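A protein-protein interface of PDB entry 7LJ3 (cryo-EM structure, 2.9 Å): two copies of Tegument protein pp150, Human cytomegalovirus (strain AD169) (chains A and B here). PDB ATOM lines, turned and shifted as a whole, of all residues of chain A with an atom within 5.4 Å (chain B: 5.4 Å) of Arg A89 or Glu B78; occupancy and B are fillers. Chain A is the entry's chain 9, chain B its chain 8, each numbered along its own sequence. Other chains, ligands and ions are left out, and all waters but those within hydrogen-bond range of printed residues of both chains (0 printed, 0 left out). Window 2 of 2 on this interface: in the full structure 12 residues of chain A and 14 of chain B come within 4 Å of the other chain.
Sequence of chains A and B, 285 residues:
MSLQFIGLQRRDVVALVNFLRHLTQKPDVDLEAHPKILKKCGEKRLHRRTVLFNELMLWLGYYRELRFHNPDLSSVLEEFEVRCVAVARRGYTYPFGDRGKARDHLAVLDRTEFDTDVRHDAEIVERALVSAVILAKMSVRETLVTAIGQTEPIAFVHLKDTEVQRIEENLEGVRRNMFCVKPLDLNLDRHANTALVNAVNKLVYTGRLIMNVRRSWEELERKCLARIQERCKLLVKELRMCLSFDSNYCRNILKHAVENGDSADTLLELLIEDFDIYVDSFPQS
1 position is printed for both chains. Of the 9 pairs that touch across the chains among the printed residues, none has its exchanged pair printed and touching as well.
Among the printed residues, merely in contact across the chains: Val A82 with Ser B74 (3.1 Å), Arg A89 with Leu B77 (3.998 Å), Arg A89 with Glu B78 (3.97 Å), Arg A89 with Phe B114 (3.6 Å) and Thr A93 with Phe B114 (3.3 Å).
Of the printed residues of chain B, Arg A89 touches Ser B74 (3.4 Å), Leu B77 (3.998 Å), Glu B78 (3.97 Å), Glu B81 (3.2 Å) and Phe B114 (3.6 Å). Of chain A, only Arg A89 comes within 4 Å of Glu B78. Of the printed residues of chain B, Thr A93 touches Phe B114 (3.3 Å) and Asp B115 (3.1 Å). Of the printed residues of chain B, Val A82 touches Ser B74. Of the printed residues of chain A, Leu B77 touches Arg A89. Of the printed residues of chain A, Ser B74 touches Val A82 (3.1 Å) and Arg A89 (3.4 Å). Of the printed residues of chain A, Glu B81 touches Arg A89 (3.2 Å). Glu B79 touches none of the printed residues of chain A. Ala A86 touches none of the printed residues of chain B.
The side-chain carboxylate of Asp B115 is in hydrogen-bond range of the side-chain hydroxyl of Thr A93, 3.1 Å away. The backbone carbonyl oxygen of Asp B115 sits at hydrogen-bond distance from the guanidinium group of Arg A90 (2.4 Å). NH1 of Arg A89 sits at hydrogen-bond distance from O of Ser B74 (3.4 Å). The guanidinium group (NH2) of Arg A89 is in salt-bridge range of the side-chain carboxylate (OE1) of Glu B81 (3.2 Å).
Hydrophobic or aromatic side chains of chain A that line the printed part of chain B: Val A82. Among the printed residues, Asp or Glu carboxylates within 4 Å of a Lys or Arg side-chain nitrogen of the other chain: Arg A89 with Glu B81 (3.2 Å).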
ATOM      1  N   VAL A  82     -12.667  -5.316  10.179  1.00  0.00           N
ATOM      2  CA  VAL A  82     -12.725  -5.831   8.814  1.00  0.00           C
ATOM      3  C   VAL A  82     -12.382  -7.316   8.784  1.00  0.00           C
ATOM      4  O   VAL A  82     -12.977  -8.091   8.026  1.00  0.00           O
ATOM      5  CB  VAL A  82     -11.810  -5.012   7.887  1.00  0.00           C
ATOM      6  CG1 VAL A  82     -11.707  -5.671   6.537  1.00  0.00           C
ATOM      7  CG2 VAL A  82     -12.352  -3.609   7.739  1.00  0.00           C
ATOM      8  N   CYS A  84     -12.975  -9.389  11.173  1.00  0.00           N
ATOM      9  CA  CYS A  84     -14.173 -10.065  11.660  1.00  0.00           C
ATOM     10  C   CYS A  84     -15.173 -10.284  10.530  1.00  0.00           C
ATOM     11  O   CYS A  84     -15.665 -11.401  10.330  1.00  0.00           O
ATOM     12  CB  CYS A  84     -14.802  -9.262  12.796  1.00  0.00           C
ATOM     13  SG  CYS A  84     -13.779  -9.153  14.265  1.00  0.00           S
ATOM     14  N   VAL A  85     -15.469  -9.235   9.762  1.00  0.00           N
ATOM     15  CA  VAL A  85     -16.420  -9.397   8.659  1.00  0.00           C
ATOM     16  C   VAL A  85     -15.892 -10.403   7.639  1.00  0.00           C
ATOM     17  O   VAL A  85     -16.664 -11.124   7.000  1.00  0.00           O
ATOM     18  CB  VAL A  85     -16.736  -8.040   8.005  1.00  0.00           C
ATOM     19  N   ALA A  86     -14.569 -10.466   7.470  1.00  0.00           N
ATOM     20  CA  ALA A  86     -13.975 -11.432   6.548  1.00  0.00           C
ATOM     21  C   ALA A  86     -14.166 -12.866   7.030  1.00  0.00           C
ATOM     22  O   ALA A  86     -14.489 -13.766   6.239  1.00  0.00           O
ATOM     23  CB  ALA A  86     -12.490 -11.124   6.371  1.00  0.00           C
ATOM     24  N   VAL A  87     -13.953 -13.101   8.324  1.00  0.00           N
ATOM     25  CA  VAL A  87     -14.209 -14.421   8.893  1.00  0.00           C
ATOM     26  C   VAL A  87     -15.665 -14.803   8.677  1.00  0.00           C
ATOM     27  O   VAL A  87     -15.982 -15.940   8.299  1.00  0.00           O
ATOM     28  CB  VAL A  87     -13.833 -14.436  10.387  1.00  0.00           C
ATOM     29  CG1 VAL A  87     -14.027 -15.810  10.977  1.00  0.00           C
ATOM     30  CG2 VAL A  87     -12.406 -13.972  10.577  1.00  0.00           C
ATOM     31  N   ALA A  88     -16.574 -13.853   8.901  1.00  0.00           N
ATOM     32  CA  ALA A  88     -17.984 -14.127   8.655  1.00  0.00           C
ATOM     33  C   ALA A  88     -18.216 -14.520   7.207  1.00  0.00           C
ATOM     34  O   ALA A  88     -18.899 -15.509   6.925  1.00  0.00           O
ATOM     35  CB  ALA A  88     -18.834 -12.912   9.015  1.00  0.00           C
ATOM     36  N   ARG A  89     -17.642 -13.764   6.272  1.00  0.00           N
ATOM     37  CA  ARG A  89     -17.864 -14.036   4.858  1.00  0.00           C
ATOM     38  C   ARG A  89     -17.382 -15.426   4.475  1.00  0.00           C
ATOM     39  O   ARG A  89     -17.980 -16.083   3.616  1.00  0.00           O
ATOM     40  CB  ARG A  89     -17.174 -12.979   4.006  1.00  0.00           C
ATOM     41  CG  ARG A  89     -16.877 -13.440   2.596  1.00  0.00           C
ATOM     42  CD  ARG A  89     -16.471 -12.291   1.692  1.00  0.00           C
ATOM     43  NE  ARG A  89     -15.438 -11.457   2.295  1.00  0.00           N
ATOM     44  CZ  ARG A  89     -15.639 -10.214   2.721  1.00  0.00           C
ATOM     45  NH1 ARG A  89     -14.646  -9.531   3.262  1.00  0.00           N
ATOM     46  NH2 ARG A  89     -16.829  -9.648   2.593  1.00  0.00           N
ATOM     47  N   ARG A  90     -16.287 -15.885   5.075  1.00  0.00           N
ATOM     48  CA  ARG A  90     -15.843 -17.241   4.766  1.00  0.00           C
ATOM     49  C   ARG A  90     -16.758 -18.284   5.396  1.00  0.00           C
ATOM     50  O   ARG A  90     -16.980 -19.351   4.816  1.00  0.00           O
ATOM     51  CB  ARG A  90     -14.401 -17.455   5.209  1.00  0.00           C
ATOM     52  CG  ARG A  90     -13.401 -16.867   4.252  1.00  0.00           C
ATOM     53  CD  ARG A  90     -13.828 -17.113   2.826  1.00  0.00           C
ATOM     54  NE  ARG A  90     -13.106 -16.253   1.900  1.00  0.00           N
ATOM     55  CZ  ARG A  90     -13.332 -16.200   0.593  1.00  0.00           C
ATOM     56  NH1 ARG A  90     -14.267 -16.954   0.045  1.00  0.00           N
ATOM     57  NH2 ARG A  90     -12.621 -15.387  -0.165  1.00  0.00           N
ATOM     58  N   GLY A  91     -17.289 -17.999   6.585  1.00  0.00           N
ATOM     59  CA  GLY A  91     -18.042 -19.015   7.309  1.00  0.00           C
ATOM     60  C   GLY A  91     -19.392 -19.341   6.695  1.00  0.00           C
ATOM     61  O   GLY A  91     -19.890 -20.457   6.838  1.00  0.00           O
ATOM     62  N   TYR A  92     -20.013 -18.372   6.022  1.00  0.00           N
ATOM     63  CA  TYR A  92     -21.437 -18.483   5.708  1.00  0.00           C
ATOM     64  C   TYR A  92     -21.765 -19.748   4.927  1.00  0.00           C
ATOM     65  O   TYR A  92     -22.596 -20.555   5.359  1.00  0.00           O
ATOM     66  CB  TYR A  92     -21.891 -17.258   4.921  1.00  0.00           C
ATOM     67  CG  TYR A  92     -22.190 -16.074   5.793  1.00  0.00           C
ATOM     68  CD1 TYR A  92     -22.926 -16.222   6.955  1.00  0.00           C
ATOM     69  CD2 TYR A  92     -21.725 -14.808   5.465  1.00  0.00           C
ATOM     70  CE1 TYR A  92     -23.192 -15.149   7.767  1.00  0.00           C
ATOM     71  CE2 TYR A  92     -21.990 -13.721   6.273  1.00  0.00           C
ATOM     72  CZ  TYR A  92     -22.725 -13.899   7.424  1.00  0.00           C
ATOM     73  OH  TYR A  92     -23.006 -12.835   8.244  1.00  0.00           O
ATOM     74  N   THR A  93     -21.124 -19.941   3.776  1.00  0.00           N
ATOM     75  CA  THR A  93     -21.548 -20.987   2.850  1.00  0.00           C
ATOM     76  C   THR A  93     -21.237 -22.379   3.381  1.00  0.00           C
ATOM     77  O   THR A  93     -21.847 -23.360   2.946  1.00  0.00           O
ATOM     78  CB  THR A  93     -20.894 -20.772   1.491  1.00  0.00           C
ATOM     79  OG1 THR A  93     -19.469 -20.795   1.648  1.00  0.00           O
ATOM     80  CG2 THR A  93     -21.305 -19.432   0.917  1.00  0.00           C
ATOM     81  N   LEU B  73      -8.253  -8.951  -0.736  1.00  0.00           N
ATOM     82  CA  LEU B  73      -9.147  -7.914  -1.223  1.00  0.00           C
ATOM     83  C   LEU B  73     -10.391  -7.765  -0.363  1.00  0.00           C
ATOM     84  O   LEU B  73     -11.442  -7.368  -0.870  1.00  0.00           O
ATOM     85  CB  LEU B  73      -9.542  -8.197  -2.668  1.00  0.00           C
ATOM     86  CG  LEU B  73      -8.413  -8.408  -3.666  1.00  0.00           C
ATOM     87  CD1 LEU B  73      -8.347  -9.859  -4.040  1.00  0.00           C
ATOM     88  CD2 LEU B  73      -8.659  -7.579  -4.891  1.00  0.00           C
ATOM     89  N   SER B  74     -10.291  -8.058   0.933  1.00  0.00           N
ATOM     90  CA  SER B  74     -11.480  -8.095   1.777  1.00  0.00           C
ATOM     91  C   SER B  74     -12.335  -6.843   1.603  1.00  0.00           C
ATOM     92  O   SER B  74     -13.549  -6.928   1.382  1.00  0.00           O
ATOM     93  CB  SER B  74     -11.072  -8.285   3.235  1.00  0.00           C
ATOM     94  OG  SER B  74     -10.997  -7.051   3.907  1.00  0.00           O
ATOM     95  N   SER B  75     -11.714  -5.670   1.683  1.00  0.00           N
ATOM     96  CA  SER B  75     -12.455  -4.436   1.455  1.00  0.00           C
ATOM     97  C   SER B  75     -13.064  -4.411   0.061  1.00  0.00           C
ATOM     98  O   SER B  75     -14.207  -3.973  -0.126  1.00  0.00           O
ATOM     99  CB  SER B  75     -11.533  -3.242   1.654  1.00  0.00           C
ATOM    100  OG  SER B  75     -12.013  -2.126   0.939  1.00  0.00           O
ATOM    101  N   VAL B  76     -12.308  -4.868  -0.934  1.00  0.00           N
ATOM    102  CA  VAL B  76     -12.810  -4.904  -2.302  1.00  0.00           C
ATOM    103  C   VAL B  76     -14.001  -5.844  -2.403  1.00  0.00           C
ATOM    104  O   VAL B  76     -14.975  -5.563  -3.109  1.00  0.00           O
ATOM    105  CB  VAL B  76     -11.679  -5.301  -3.262  1.00  0.00           C
ATOM    106  CG1 VAL B  76     -12.113  -5.139  -4.702  1.00  0.00           C
ATOM    107  CG2 VAL B  76     -10.473  -4.449  -2.987  1.00  0.00           C
ATOM    108  N   LEU B  77     -13.954  -6.963  -1.681  1.00  0.00           N
ATOM    109  CA  LEU B  77     -15.061  -7.913  -1.711  1.00  0.00           C
ATOM    110  C   LEU B  77     -16.315  -7.330  -1.069  1.00  0.00           C
ATOM    111  O   LEU B  77     -17.429  -7.505  -1.584  1.00  0.00           O
ATOM    112  CB  LEU B  77     -14.648  -9.210  -1.020  1.00  0.00           C
ATOM    113  CG  LEU B  77     -13.563  -9.998  -1.746  1.00  0.00           C
ATOM    114  CD1 LEU B  77     -12.423 -10.289  -0.818  1.00  0.00           C
ATOM    115  CD2 LEU B  77     -14.142 -11.281  -2.248  1.00  0.00           C
ATOM    116  N   GLU B  78     -16.163  -6.650   0.070  1.00  0.00           N
ATOM    117  CA  GLU B  78     -17.326  -6.036   0.700  1.00  0.00           C
ATOM    118  C   GLU B  78     -17.892  -4.917  -0.165  1.00  0.00           C
ATOM    119  O   GLU B  78     -19.100  -4.661  -0.149  1.00  0.00           O
ATOM    120  CB  GLU B  78     -16.983  -5.519   2.092  1.00  0.00           C
ATOM    121  CG  GLU B  78     -18.222  -5.103   2.848  1.00  0.00           C
ATOM    122  CD  GLU B  78     -17.950  -4.805   4.297  1.00  0.00           C
ATOM    123  OE1 GLU B  78     -16.761  -4.752   4.678  1.00  0.00           O
ATOM    124  OE2 GLU B  78     -18.929  -4.629   5.055  1.00  0.00           O
ATOM    125  N   GLU B  79     -17.031  -4.219  -0.904  1.00  0.00           N
ATOM    126  CA  GLU B  79     -17.516  -3.264  -1.895  1.00  0.00           C
ATOM    127  C   GLU B  79     -18.305  -3.963  -2.997  1.00  0.00           C
ATOM    128  O   GLU B  79     -19.358  -3.475  -3.429  1.00  0.00           O
ATOM    129  CB  GLU B  79     -16.335  -2.499  -2.481  1.00  0.00           C
ATOM    130  CG  GLU B  79     -16.712  -1.371  -3.403  1.00  0.00           C
ATOM    131  CD  GLU B  79     -16.476  -0.006  -2.790  1.00  0.00           C
ATOM    132  OE1 GLU B  79     -16.122   0.061  -1.593  1.00  0.00           O
ATOM    133  OE2 GLU B  79     -16.643   0.999  -3.507  1.00  0.00           O
ATOM    134  N   PHE B  80     -17.811  -5.113  -3.459  1.00  0.00           N
ATOM    135  CA  PHE B  80     -18.456  -5.813  -4.563  1.00  0.00           C
ATOM    136  C   PHE B  80     -19.847  -6.292  -4.184  1.00  0.00           C
ATOM    137  O   PHE B  80     -20.783  -6.188  -4.982  1.00  0.00           O
ATOM    138  CB  PHE B  80     -17.596  -6.993  -5.010  1.00  0.00           C
ATOM    139  CG  PHE B  80     -18.224  -7.826  -6.090  1.00  0.00           C
ATOM    140  CD1 PHE B  80     -18.195  -7.413  -7.407  1.00  0.00           C
ATOM    141  CD2 PHE B  80     -18.836  -9.030  -5.791  1.00  0.00           C
ATOM    142  CE1 PHE B  80     -18.765  -8.174  -8.397  1.00  0.00           C
ATOM    143  CE2 PHE B  80     -19.409  -9.799  -6.785  1.00  0.00           C
ATOM    144  CZ  PHE B  80     -19.374  -9.370  -8.085  1.00  0.00           C
ATOM    145  N   GLU B  81     -20.001  -6.843  -2.980  1.00  0.00           N
ATOM    146  CA  GLU B  81     -21.316  -7.336  -2.575  1.00  0.00           C
ATOM    147  C   GLU B  81     -22.333  -6.200  -2.514  1.00  0.00           C
ATOM    148  O   GLU B  81     -23.471  -6.338  -2.987  1.00  0.00           O
ATOM    149  CB  GLU B  81     -21.215  -8.060  -1.234  1.00  0.00           C
ATOM    150  CG  GLU B  81     -20.603  -9.443  -1.354  1.00  0.00           C
ATOM    151  CD  GLU B  81     -20.154 -10.028  -0.032  1.00  0.00           C
ATOM    152  OE1 GLU B  81     -19.416  -9.347   0.699  1.00  0.00           O
ATOM    153  OE2 GLU B  81     -20.533 -11.178   0.274  1.00  0.00           O
ATOM    154  N   VAL B  82     -21.928  -5.055  -1.964  1.00  0.00           N
ATOM    155  CA  VAL B  82     -22.827  -3.908  -1.887  1.00  0.00           C
ATOM    156  C   VAL B  82     -23.214  -3.434  -3.280  1.00  0.00           C
ATOM    157  O   VAL B  82     -24.389  -3.158  -3.550  1.00  0.00           O
ATOM    158  CB  VAL B  82     -22.181  -2.777  -1.073  1.00  0.00           C
ATOM    159  CG1 VAL B  82     -22.958  -1.497  -1.262  1.00  0.00           C
ATOM    160  CG2 VAL B  82     -22.127  -3.152   0.384  1.00  0.00           C
ATOM    161  N   ARG B  83     -22.239  -3.324  -4.184  1.00  0.00           N
ATOM    162  CA  ARG B  83     -22.545  -2.816  -5.519  1.00  0.00           C
ATOM    163  C   ARG B  83     -23.395  -3.803  -6.308  1.00  0.00           C
ATOM    164  O   ARG B  83     -24.224  -3.401  -7.131  1.00  0.00           O
ATOM    165  CB  ARG B  83     -21.257  -2.471  -6.256  1.00  0.00           C
ATOM    166  CG  ARG B  83     -20.565  -1.275  -5.650  1.00  0.00           C
ATOM    167  CD  ARG B  83     -19.296  -0.907  -6.366  1.00  0.00           C
ATOM    168  NE  ARG B  83     -18.667   0.246  -5.729  1.00  0.00           N
ATOM    169  CZ  ARG B  83     -17.597   0.873  -6.201  1.00  0.00           C
ATOM    170  NH1 ARG B  83     -17.029   0.467  -7.323  1.00  0.00           N
ATOM    171  NH2 ARG B  83     -17.094   1.908  -5.547  1.00  0.00           N
ATOM    172  N   PHE B 114     -19.824 -15.334  -2.102  1.00  0.00           N
ATOM    173  CA  PHE B 114     -18.508 -15.949  -2.062  1.00  0.00           C
ATOM    174  C   PHE B 114     -18.537 -17.251  -1.272  1.00  0.00           C
ATOM    175  O   PHE B 114     -19.069 -17.302  -0.161  1.00  0.00           O
ATOM    176  CB  PHE B 114     -17.487 -14.983  -1.467  1.00  0.00           C
ATOM    177  CG  PHE B 114     -17.330 -13.724  -2.260  1.00  0.00           C
ATOM    178  CD1 PHE B 114     -16.926 -13.775  -3.580  1.00  0.00           C
ATOM    179  CD2 PHE B 114     -17.588 -12.491  -1.694  1.00  0.00           C
ATOM    180  CE1 PHE B 114     -16.788 -12.626  -4.321  1.00  0.00           C
ATOM    181  CE2 PHE B 114     -17.443 -11.337  -2.437  1.00  0.00           C
ATOM    182  CZ  PHE B 114     -17.048 -11.408  -3.750  1.00  0.00           C
ATOM    183  N   ASP B 115     -17.962 -18.291  -1.865  1.00  0.00           N
ATOM    184  CA  ASP B 115     -17.820 -19.602  -1.259  1.00  0.00           C
ATOM    185  C   ASP B 115     -16.727 -19.589  -0.193  1.00  0.00           C
ATOM    186  O   ASP B 115     -16.089 -18.570   0.076  1.00  0.00           O
ATOM    187  CB  ASP B 115     -17.490 -20.639  -2.334  1.00  0.00           C
ATOM    188  CG  ASP B 115     -17.623 -22.068  -1.842  1.00  0.00           C
ATOM    189  OD1 ASP B 115     -18.116 -22.270  -0.713  1.00  0.00           O
ATOM    190  OD2 ASP B 115     -17.226 -22.993  -2.579  1.00  0.00           O
